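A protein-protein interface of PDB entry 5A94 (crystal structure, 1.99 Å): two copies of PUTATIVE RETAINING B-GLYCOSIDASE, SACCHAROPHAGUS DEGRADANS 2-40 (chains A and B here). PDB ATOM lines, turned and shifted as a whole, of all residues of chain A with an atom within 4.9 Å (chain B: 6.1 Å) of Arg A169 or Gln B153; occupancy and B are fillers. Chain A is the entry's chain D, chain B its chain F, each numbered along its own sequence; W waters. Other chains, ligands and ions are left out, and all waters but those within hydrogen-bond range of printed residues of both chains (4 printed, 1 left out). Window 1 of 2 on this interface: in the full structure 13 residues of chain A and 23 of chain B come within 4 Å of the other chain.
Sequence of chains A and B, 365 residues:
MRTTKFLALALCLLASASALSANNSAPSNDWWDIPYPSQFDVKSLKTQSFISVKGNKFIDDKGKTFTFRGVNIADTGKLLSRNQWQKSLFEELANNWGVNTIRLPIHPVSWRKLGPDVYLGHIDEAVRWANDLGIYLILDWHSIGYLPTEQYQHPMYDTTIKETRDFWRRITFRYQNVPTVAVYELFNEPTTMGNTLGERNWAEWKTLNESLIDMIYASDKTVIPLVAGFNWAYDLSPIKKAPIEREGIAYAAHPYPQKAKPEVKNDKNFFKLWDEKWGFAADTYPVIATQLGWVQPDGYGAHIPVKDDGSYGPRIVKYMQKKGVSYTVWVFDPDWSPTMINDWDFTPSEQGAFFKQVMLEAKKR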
ATOM      1  N   TYR A  36      23.547 -20.661  18.974  1.00  0.00           N
ATOM      2  CA  TYR A  36      22.377 -19.931  19.431  1.00  0.00           C
ATOM      3  C   TYR A  36      21.190 -20.886  19.573  1.00  0.00           C
ATOM      4  O   TYR A  36      21.124 -21.897  18.862  1.00  0.00           O
ATOM      5  CB  TYR A  36      22.043 -18.789  18.447  1.00  0.00           C
ATOM      6  CG  TYR A  36      22.877 -17.564  18.727  1.00  0.00           C
ATOM      7  CD1 TYR A  36      24.187 -17.469  18.269  1.00  0.00           C
ATOM      8  CD2 TYR A  36      22.379 -16.529  19.503  1.00  0.00           C
ATOM      9  CE1 TYR A  36      24.977 -16.364  18.564  1.00  0.00           C
ATOM     10  CE2 TYR A  36      23.150 -15.414  19.785  1.00  0.00           C
ATOM     11  CZ  TYR A  36      24.448 -15.339  19.321  1.00  0.00           C
ATOM     12  OH  TYR A  36      25.235 -14.254  19.629  1.00  0.00           O
ATOM     13  N   ARG A 165      14.387 -14.861  35.511  1.00  0.00           N
ATOM     14  CA  ARG A 165      14.247 -14.166  34.230  1.00  0.00           C
ATOM     15  C   ARG A 165      14.743 -15.029  33.071  1.00  0.00           C
ATOM     16  O   ARG A 165      14.087 -15.116  32.029  1.00  0.00           O
ATOM     17  CB  ARG A 165      15.041 -12.865  34.217  1.00  0.00           C
ATOM     18  CG  ARG A 165      14.487 -11.755  35.070  1.00  0.00           C
ATOM     19  CD  ARG A 165      15.328 -10.508  34.882  1.00  0.00           C
ATOM     20  NE  ARG A 165      14.952  -9.407  35.769  1.00  0.00           N
ATOM     21  CZ  ARG A 165      13.898  -8.619  35.580  1.00  0.00           C
ATOM     22  NH1 ARG A 165      13.082  -8.804  34.532  1.00  0.00           N
ATOM     23  NH2 ARG A 165      13.643  -7.638  36.437  1.00  0.00           N
ATOM     24  N   ASP A 166      15.899 -15.647  33.257  1.00  0.00           N
ATOM     25  CA  ASP A 166      16.524 -16.453  32.219  1.00  0.00           C
ATOM     26  C   ASP A 166      15.698 -17.694  31.899  1.00  0.00           C
ATOM     27  O   ASP A 166      15.561 -18.068  30.736  1.00  0.00           O
ATOM     28  CB  ASP A 166      17.939 -16.878  32.610  1.00  0.00           C
ATOM     29  CG  ASP A 166      18.568 -17.773  31.573  1.00  0.00           C
ATOM     30  OD1 ASP A 166      18.890 -17.275  30.488  1.00  0.00           O
ATOM     31  OD2 ASP A 166      18.682 -19.005  31.816  1.00  0.00           O
ATOM     32  N   PHE A 167      15.116 -18.313  32.931  1.00  0.00           N
ATOM     33  CA  PHE A 167      14.199 -19.413  32.720  1.00  0.00           C
ATOM     34  C   PHE A 167      13.042 -18.980  31.815  1.00  0.00           C
ATOM     35  O   PHE A 167      12.750 -19.640  30.829  1.00  0.00           O
ATOM     36  CB  PHE A 167      13.659 -19.953  34.054  1.00  0.00           C
ATOM     37  CG  PHE A 167      12.575 -20.962  33.891  1.00  0.00           C
ATOM     38  CD1 PHE A 167      12.868 -22.258  33.519  1.00  0.00           C
ATOM     39  CD2 PHE A 167      11.240 -20.618  34.097  1.00  0.00           C
ATOM     40  CE1 PHE A 167      11.869 -23.201  33.363  1.00  0.00           C
ATOM     41  CE2 PHE A 167      10.238 -21.561  33.927  1.00  0.00           C
ATOM     42  CZ  PHE A 167      10.551 -22.851  33.567  1.00  0.00           C
ATOM     43  N   TRP A 168      12.401 -17.874  32.150  1.00  0.00           N
ATOM     44  CA  TRP A 168      11.282 -17.419  31.336  1.00  0.00           C
ATOM     45  C   TRP A 168      11.701 -16.915  29.949  1.00  0.00           C
ATOM     46  O   TRP A 168      10.951 -17.071  28.986  1.00  0.00           O
ATOM     47  CB  TRP A 168      10.437 -16.391  32.080  1.00  0.00           C
ATOM     48  CG  TRP A 168       9.696 -17.041  33.202  1.00  0.00           C
ATOM     49  CD1 TRP A 168       9.830 -16.779  34.537  1.00  0.00           C
ATOM     50  CD2 TRP A 168       8.746 -18.103  33.092  1.00  0.00           C
ATOM     51  NE1 TRP A 168       9.002 -17.597  35.263  1.00  0.00           N
ATOM     52  CE2 TRP A 168       8.324 -18.424  34.405  1.00  0.00           C
ATOM     53  CE3 TRP A 168       8.215 -18.816  32.023  1.00  0.00           C
ATOM     54  CZ2 TRP A 168       7.397 -19.412  34.661  1.00  0.00           C
ATOM     55  CZ3 TRP A 168       7.285 -19.822  32.288  1.00  0.00           C
ATOM     56  CH2 TRP A 168       6.905 -20.119  33.595  1.00  0.00           C
ATOM     57  N   ARG A 169      12.880 -16.329  29.843  1.00  0.00           N
ATOM     58  CA  ARG A 169      13.405 -15.921  28.529  1.00  0.00           C
ATOM     59  C   ARG A 169      13.525 -17.155  27.628  1.00  0.00           C
ATOM     60  O   ARG A 169      13.037 -17.167  26.493  1.00  0.00           O
ATOM     61  CB  ARG A 169      14.755 -15.234  28.696  1.00  0.00           C
ATOM     62  CG  ARG A 169      15.432 -14.800  27.407  1.00  0.00           C
ATOM     63  CD  ARG A 169      16.270 -15.909  26.811  1.00  0.00           C
ATOM     64  NE  ARG A 169      17.020 -15.432  25.659  1.00  0.00           N
ATOM     65  CZ  ARG A 169      18.135 -14.718  25.728  1.00  0.00           C
ATOM     66  NH1 ARG A 169      18.623 -14.334  26.891  1.00  0.00           N
ATOM     67  NH2 ARG A 169      18.741 -14.338  24.602  1.00  0.00           N
ATOM     68  N   ARG A 170      14.135 -18.213  28.158  1.00  0.00           N
ATOM     69  CA  ARG A 170      14.383 -19.444  27.403  1.00  0.00           C
ATOM     70  C   ARG A 170      13.091 -20.177  27.023  1.00  0.00           C
ATOM     71  O   ARG A 170      12.946 -20.661  25.889  1.00  0.00           O
ATOM     72  CB  ARG A 170      15.235 -20.407  28.228  1.00  0.00           C
ATOM     73  CG  ARG A 170      16.697 -20.027  28.372  1.00  0.00           C
ATOM     74  CD  ARG A 170      17.327 -21.020  29.321  1.00  0.00           C
ATOM     75  NE  ARG A 170      18.709 -20.739  29.656  1.00  0.00           N
ATOM     76  CZ  ARG A 170      19.765 -21.286  29.068  1.00  0.00           C
ATOM     77  NH1 ARG A 170      19.634 -22.127  28.038  1.00  0.00           N
ATOM     78  NH2 ARG A 170      20.979 -20.988  29.520  1.00  0.00           N
ATOM     79  N   ILE A 171      12.180 -20.278  27.986  1.00  0.00           N
ATOM     80  CA  ILE A 171      10.896 -20.951  27.796  1.00  0.00           C
ATOM     81  C   ILE A 171      10.085 -20.227  26.736  1.00  0.00           C
ATOM     82  O   ILE A 171       9.618 -20.845  25.775  1.00  0.00           O
ATOM     83  CB  ILE A 171      10.113 -21.010  29.126  1.00  0.00           C
ATOM     84  CG1 ILE A 171      10.764 -22.029  30.088  1.00  0.00           C
ATOM     85  CG2 ILE A 171       8.657 -21.351  28.883  1.00  0.00           C
ATOM     86  CD1 ILE A 171      10.760 -23.471  29.636  1.00  0.00           C
ATOM     87  N   THR A 172       9.958 -18.915  26.880  1.00  0.00           N
ATOM     88  CA  THR A 172       9.177 -18.132  25.940  1.00  0.00           C
ATOM     89  C   THR A 172       9.694 -18.212  24.501  1.00  0.00           C
ATOM     90  O   THR A 172       8.911 -18.324  23.546  1.00  0.00           O
ATOM     91  CB  THR A 172       9.130 -16.657  26.350  1.00  0.00           C
ATOM     92  OG1 THR A 172       8.660 -16.553  27.687  1.00  0.00           O
ATOM     93  CG2 THR A 172       8.174 -15.881  25.457  1.00  0.00           C
ATOM     94  N   PHE A 173      11.007 -18.145  24.346  1.00  0.00           N
ATOM     95  CA  PHE A 173      11.618 -18.261  23.039  1.00  0.00           C
ATOM     96  C   PHE A 173      11.373 -19.658  22.460  1.00  0.00           C
ATOM     97  O   PHE A 173      10.939 -19.788  21.310  1.00  0.00           O
ATOM     98  CB  PHE A 173      13.111 -17.948  23.116  1.00  0.00           C
ATOM     99  CG  PHE A 173      13.830 -18.106  21.824  1.00  0.00           C
ATOM    100  CD1 PHE A 173      13.708 -17.150  20.815  1.00  0.00           C
ATOM    101  CD2 PHE A 173      14.605 -19.235  21.588  1.00  0.00           C
ATOM    102  CE1 PHE A 173      14.367 -17.308  19.611  1.00  0.00           C
ATOM    103  CE2 PHE A 173      15.278 -19.386  20.387  1.00  0.00           C
ATOM    104  CZ  PHE A 173      15.149 -18.425  19.392  1.00  0.00           C
ATOM    105  N   MET A 215       8.879  -9.192  29.582  1.00  0.00           N
ATOM    106  CA  MET A 215       9.868 -10.024  28.864  1.00  0.00           C
ATOM    107  C   MET A 215       9.172 -11.113  28.061  1.00  0.00           C
ATOM    108  O   MET A 215       9.573 -11.428  26.944  1.00  0.00           O
ATOM    109  CB  MET A 215      10.809 -10.742  29.834  1.00  0.00           C
ATOM    110  CG  MET A 215      11.841  -9.879  30.534  1.00  0.00           C
ATOM    111  SD  MET A 215      12.786 -10.892  31.693  1.00  0.00           S
ATOM    112  CE  MET A 215      13.809 -11.839  30.579  1.00  0.00           C
ATOM    113  N   ILE B 144      27.035  -8.404  25.473  1.00  0.00           N
ATOM    114  CA  ILE B 144      25.934  -7.919  24.655  1.00  0.00           C
ATOM    115  C   ILE B 144      24.624  -8.236  25.371  1.00  0.00           C
ATOM    116  O   ILE B 144      24.334  -9.397  25.680  1.00  0.00           O
ATOM    117  CB  ILE B 144      25.919  -8.575  23.258  1.00  0.00           C
ATOM    118  CG1 ILE B 144      27.277  -8.427  22.564  1.00  0.00           C
ATOM    119  CG2 ILE B 144      24.812  -7.958  22.403  1.00  0.00           C
ATOM    120  CD1 ILE B 144      27.350  -9.173  21.257  1.00  0.00           C
ATOM    121  N   GLY B 145      23.879  -7.196  25.725  1.00  0.00           N
ATOM    122  CA  GLY B 145      22.643  -7.375  26.470  1.00  0.00           C
ATOM    123  C   GLY B 145      22.352  -6.248  27.429  1.00  0.00           C
ATOM    124  O   GLY B 145      22.846  -5.137  27.266  1.00  0.00           O
ATOM    125  N   GLN B 151      20.588  -9.987  31.719  1.00  0.00           N
ATOM    126  CA  GLN B 151      20.148 -10.882  30.662  1.00  0.00           C
ATOM    127  C   GLN B 151      20.880 -10.523  29.374  1.00  0.00           C
ATOM    128  O   GLN B 151      21.065  -9.344  29.071  1.00  0.00           O
ATOM    129  CB  GLN B 151      18.643 -10.752  30.435  1.00  0.00           C
ATOM    130  CG  GLN B 151      17.807 -10.872  31.676  1.00  0.00           C
ATOM    131  CD  GLN B 151      17.846 -12.259  32.279  1.00  0.00           C
ATOM    132  OE1 GLN B 151      17.402 -13.220  31.656  1.00  0.00           O
ATOM    133  NE2 GLN B 151      18.334 -12.365  33.494  1.00  0.00           N
ATOM    134  N   TYR B 152      21.287 -11.538  28.610  1.00  0.00           N
ATOM    135  CA  TYR B 152      22.256 -11.343  27.513  1.00  0.00           C
ATOM    136  C   TYR B 152      21.898 -12.087  26.236  1.00  0.00           C
ATOM    137  O   TYR B 152      21.053 -12.992  26.222  1.00  0.00           O
ATOM    138  CB  TYR B 152      23.672 -11.730  27.977  1.00  0.00           C
ATOM    139  CG  TYR B 152      24.030 -11.056  29.278  1.00  0.00           C
ATOM    140  CD1 TYR B 152      24.514  -9.752  29.296  1.00  0.00           C
ATOM    141  CD2 TYR B 152      23.794 -11.691  30.486  1.00  0.00           C
ATOM    142  CE1 TYR B 152      24.791  -9.119  30.479  1.00  0.00           C
ATOM    143  CE2 TYR B 152      24.068 -11.070  31.676  1.00  0.00           C
ATOM    144  CZ  TYR B 152      24.564  -9.784  31.678  1.00  0.00           C
ATOM    145  OH  TYR B 152      24.819  -9.166  32.852  1.00  0.00           O
ATOM    146  N   GLN B 153      22.516 -11.656  25.144  1.00  0.00           N
ATOM    147  CA  GLN B 153      22.245 -12.222  23.815  1.00  0.00           C
ATOM    148  C   GLN B 153      22.682 -13.672  23.699  1.00  0.00           C
ATOM    149  O   GLN B 153      22.045 -14.451  22.990  1.00  0.00           O
ATOM    150  CB  GLN B 153      22.943 -11.386  22.740  1.00  0.00           C
ATOM    151  CG  GLN B 153      22.808 -11.927  21.338  1.00  0.00           C
ATOM    152  CD  GLN B 153      23.307 -10.939  20.302  1.00  0.00           C
ATOM    153  OE1 GLN B 153      22.747  -9.868  20.147  1.00  0.00           O
ATOM    154  NE2 GLN B 153      24.374 -11.304  19.584  1.00  0.00           N
ATOM    155  N   HIS B 154      23.747 -14.025  24.406  1.00  0.00           N
ATOM    156  CA  HIS B 154      24.354 -15.368  24.317  1.00  0.00           C
ATOM    157  C   HIS B 154      25.139 -15.645  25.613  1.00  0.00           C
ATOM    158  O   HIS B 154      25.636 -14.703  26.213  1.00  0.00           O
ATOM    159  CB  HIS B 154      25.291 -15.418  23.117  1.00  0.00           C
ATOM    160  CG  HIS B 154      25.829 -16.780  22.824  1.00  0.00           C
ATOM    161  ND1 HIS B 154      26.844 -17.344  23.558  1.00  0.00           N
ATOM    162  CD2 HIS B 154      25.511 -17.688  21.873  1.00  0.00           C
ATOM    163  CE1 HIS B 154      27.127 -18.539  23.083  1.00  0.00           C
ATOM    164  NE2 HIS B 154      26.322 -18.776  22.065  1.00  0.00           N
ATOM    165  N   PRO B 155      25.234 -16.926  26.043  1.00  0.00           N
ATOM    166  CA  PRO B 155      25.917 -17.205  27.319  1.00  0.00           C
ATOM    167  C   PRO B 155      27.396 -16.788  27.333  1.00  0.00           C
ATOM    168  O   PRO B 155      27.918 -16.502  28.388  1.00  0.00           O
ATOM    169  CB  PRO B 155      25.798 -18.721  27.462  1.00  0.00           C
ATOM    170  CG  PRO B 155      24.615 -19.090  26.665  1.00  0.00           C
ATOM    171  CD  PRO B 155      24.569 -18.132  25.513  1.00  0.00           C
ATOM    172  N   TYR B 157      28.481 -14.050  26.680  1.00  0.00           N
ATOM    173  CA  TYR B 157      28.460 -12.677  27.202  1.00  0.00           C
ATOM    174  C   TYR B 157      27.917 -12.574  28.622  1.00  0.00           C
ATOM    175  O   TYR B 157      27.830 -11.469  29.195  1.00  0.00           O
ATOM    176  CB  TYR B 157      27.621 -11.783  26.283  1.00  0.00           C
ATOM    177  CG  TYR B 157      28.008 -11.912  24.817  1.00  0.00           C
ATOM    178  CD1 TYR B 157      29.301 -11.620  24.381  1.00  0.00           C
ATOM    179  CD2 TYR B 157      27.090 -12.349  23.879  1.00  0.00           C
ATOM    180  CE1 TYR B 157      29.647 -11.728  23.041  1.00  0.00           C
ATOM    181  CE2 TYR B 157      27.418 -12.458  22.537  1.00  0.00           C
ATOM    182  CZ  TYR B 157      28.694 -12.147  22.121  1.00  0.00           C
ATOM    183  OH  TYR B 157      29.003 -12.285  20.785  1.00  0.00           O
ATOM    184  N   GLU B 189      28.032  -3.666  24.165  1.00  0.00           N
ATOM    185  CA  GLU B 189      26.807  -3.457  23.424  1.00  0.00           C
ATOM    186  C   GLU B 189      25.528  -3.567  24.255  1.00  0.00           C
ATOM    187  O   GLU B 189      24.899  -4.636  24.318  1.00  0.00           O
ATOM    188  CB  GLU B 189      26.759  -4.393  22.211  1.00  0.00           C
ATOM    189  CG  GLU B 189      27.542  -3.817  21.043  1.00  0.00           C
ATOM    190  CD  GLU B 189      27.500  -4.644  19.779  1.00  0.00           C
ATOM    191  OE1 GLU B 189      27.117  -5.831  19.822  1.00  0.00           O
ATOM    192  OE2 GLU B 189      27.897  -4.096  18.717  1.00  0.00           O
ATOM    193  N   THR B 191      21.854  -3.671  24.790  1.00  0.00           N
ATOM    194  CA  THR B 191      20.637  -3.935  24.022  1.00  0.00           C
ATOM    195  C   THR B 191      19.665  -4.735  24.892  1.00  0.00           C
ATOM    196  O   THR B 191      20.083  -5.521  25.753  1.00  0.00           O
ATOM    197  CB  THR B 191      20.936  -4.721  22.734  1.00  0.00           C
ATOM    198  OG1 THR B 191      19.722  -4.969  22.027  1.00  0.00           O
ATOM    199  CG2 THR B 191      21.626  -6.062  23.045  1.00  0.00           C
ATOM    200  N   MET B 193      17.292  -6.409  23.031  1.00  0.00           N
ATOM    201  CA  MET B 193      16.774  -7.284  21.962  1.00  0.00           C
ATOM    202  C   MET B 193      15.254  -7.172  21.845  1.00  0.00           C
ATOM    203  O   MET B 193      14.516  -8.150  22.053  1.00  0.00           O
ATOM    204  CB  MET B 193      17.180  -8.750  22.206  1.00  0.00           C
ATOM    205  CG  MET B 193      18.683  -9.004  22.228  1.00  0.00           C
ATOM    206  SD  MET B 193      19.113 -10.759  22.483  1.00  0.00           S
ATOM    207  CE  MET B 193      18.657 -11.434  20.883  1.00  0.00           C
ATOM    208  N   THR B 196      13.040  -8.040  24.940  1.00  0.00           N
ATOM    209  CA  THR B 196      13.000  -9.423  25.390  1.00  0.00           C
ATOM    210  C   THR B 196      13.941  -9.695  26.578  1.00  0.00           C
ATOM    211  O   THR B 196      13.739 -10.672  27.318  1.00  0.00           O
ATOM    212  CB  THR B 196      13.342 -10.420  24.260  1.00  0.00           C
ATOM    213  OG1 THR B 196      14.661 -10.157  23.759  1.00  0.00           O
ATOM    214  CG2 THR B 196      12.321 -10.351  23.148  1.00  0.00           C
ATOM    215  N   LEU B 197      14.965  -8.845  26.761  1.00  0.00           N
ATOM    216  CA  LEU B 197      15.918  -8.999  27.867  1.00  0.00           C
ATOM    217  C   LEU B 197      15.580  -8.163  29.096  1.00  0.00           C
ATOM    218  O   LEU B 197      16.213  -8.308  30.156  1.00  0.00           O
ATOM    219  CB  LEU B 197      17.333  -8.658  27.405  1.00  0.00           C
ATOM    220  CG  LEU B 197      17.860  -9.435  26.208  1.00  0.00           C
ATOM    221  CD1 LEU B 197      19.309  -9.085  25.938  1.00  0.00           C
ATOM    222  CD2 LEU B 197      17.720 -10.935  26.431  1.00  0.00           C
ATOM    223  N   TRP B 232      22.445  -1.967  20.515  1.00  0.00           N
ATOM    224  CA  TRP B 232      23.779  -2.482  20.320  1.00  0.00           C
ATOM    225  C   TRP B 232      24.794  -1.357  20.144  1.00  0.00           C
ATOM    226  O   TRP B 232      25.591  -1.369  19.194  1.00  0.00           O
ATOM    227  CB  TRP B 232      23.840  -3.438  19.137  1.00  0.00           C
ATOM    228  CG  TRP B 232      23.157  -4.755  19.348  1.00  0.00           C
ATOM    229  CD1 TRP B 232      23.750  -5.922  19.720  1.00  0.00           C
ATOM    230  CD2 TRP B 232      21.775  -5.051  19.150  1.00  0.00           C
ATOM    231  NE1 TRP B 232      22.831  -6.920  19.781  1.00  0.00           N
ATOM    232  CE2 TRP B 232      21.605  -6.418  19.435  1.00  0.00           C
ATOM    233  CE3 TRP B 232      20.662  -4.295  18.759  1.00  0.00           C
ATOM    234  CZ2 TRP B 232      20.379  -7.055  19.331  1.00  0.00           C
ATOM    235  CZ3 TRP B 232      19.435  -4.923  18.679  1.00  0.00           C
ATOM    236  CH2 TRP B 232      19.299  -6.291  18.973  1.00  0.00           C
HETATM  237  O   HOH W   1      18.377 -14.961  29.624  1.00  0.00           O
HETATM  238  O   HOH W   2      16.285 -12.431  23.119  1.00  0.00           O
HETATM  239  O   HOH W   3      11.988 -12.869  26.756  1.00  0.00           O
HETATM  240  O   HOH W   4      21.006 -16.661  25.052  1.00  0.00           O
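The side-chain hydroxyl (OH) of Tyr A36 sits at hydrogen-bond distance from the side-chain amide nitrogen (NE2) of Gln B153 (3.1 Å). The side-chain amide oxygen (OE1) of Gln B151 sits at hydrogen-bond distance from the backbone NH (N) of Asp A166 (3.3 Å). The guanidinium group (NH1) of Arg A169 lies within hydrogen-bond range of the backbone carbonyl oxygen (O) of Tyr B152, at 2.9 Å.
The guanidinium group of Arg A165 sits at hydrogen-bond distance from the side-chain sulfur of Met A215 (3.5 Å). The side-chain carboxylate of Asp A166 lies within salt-bridge range of the guanidinium group of Arg A170 (2.8 Å). O of Ile B144 sits at hydrogen-bond distance from N of Gln B153 (2.9 Å). OE1 of Gln B153 sits at hydrogen-bond distance from NE1 of Trp B232 (3.0 Å). O of Met B193 is in hydrogen-bond range of OG1 of Thr B196 (2.6 Å).
Among the printed residues, merely in contact across the chains: Arg A165 with Gln B151 (3.4 Å), Met A215 with Thr B196 (3.5 Å), Arg A169 with Leu B197 (3.5 Å), Tyr A36 with His B154 (3.6 Å), Arg A169 with Gln B153 (3.7 Å) and Met A215 with Gln B151 (3.997 Å).
Arg A169 touches just these residues of chain B: Tyr B152 (2.9 Å), Gln B153 (3.7 Å) and Leu B197 (3.5 Å). Of the printed residues of chain B, Asp A166 touches Gln B151 (3.3 Å). Of the printed residues of chain A, Leu B197 touches Arg A169 (3.5 Å). Printed residues of chain A within 4 Å of Gln B151: Arg A165 (3.4 Å), Asp A166 (3.3 Å) and Met A215 (3.997 Å). Trp B232 touches none of the printed residues of chain A. Glu B189 touches none of the printed residues of chain A. The nearest residue of chain B that does not touch Arg A169 is Met B193 (4.2 Å). The nearest printed residue of chain A that does not touch Gln B153 is Asp A166 (8.6 Å).
Hydrophobic or aromatic side chains of chain A within 4 Å of the printed part of chain B: Tyr A36 and Met A215. Of the 14 printed residues of chain B, 6 touch a printed residue of chain A. Hydrophobic or aromatic side chains of chain B that line the printed part of chain A: His B154 and Leu B197. Among the printed residues, 9 pairs touch across the chains. Among the printed residues, no Asp or Glu carboxylate lies within 4 Å of a Lys or Arg side-chain nitrogen of the other chain.
No position is printed for both chains. Of the 9 pairs that touch across the chains among the printed residues, none has its exchanged pair printed and touching as well.
Water W1 lies within hydrogen-bond range of OD1 of Asp A166 (2.5 Å), NH1 of Arg A169 (2.8 Å) and OE1 of Gln B151 (2.8 Å). Water W3 lies within hydrogen-bond range of the backbone carbonyl oxygen of Met A215 (2.8 Å) and the backbone carbonyl oxygen of Thr B196 (2.9 Å). Water W2 lies within hydrogen-bond range of OG1 of Thr B196 (2.9 Å), SD of Met B193 (3.3 Å) and NH2 of Arg A169 (3.4 Å). Water W4 bridges the backbone carbonyl oxygen of Gln B153 (3.2 Å) and the guanidinium group of Arg A169 (3.3 Å).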
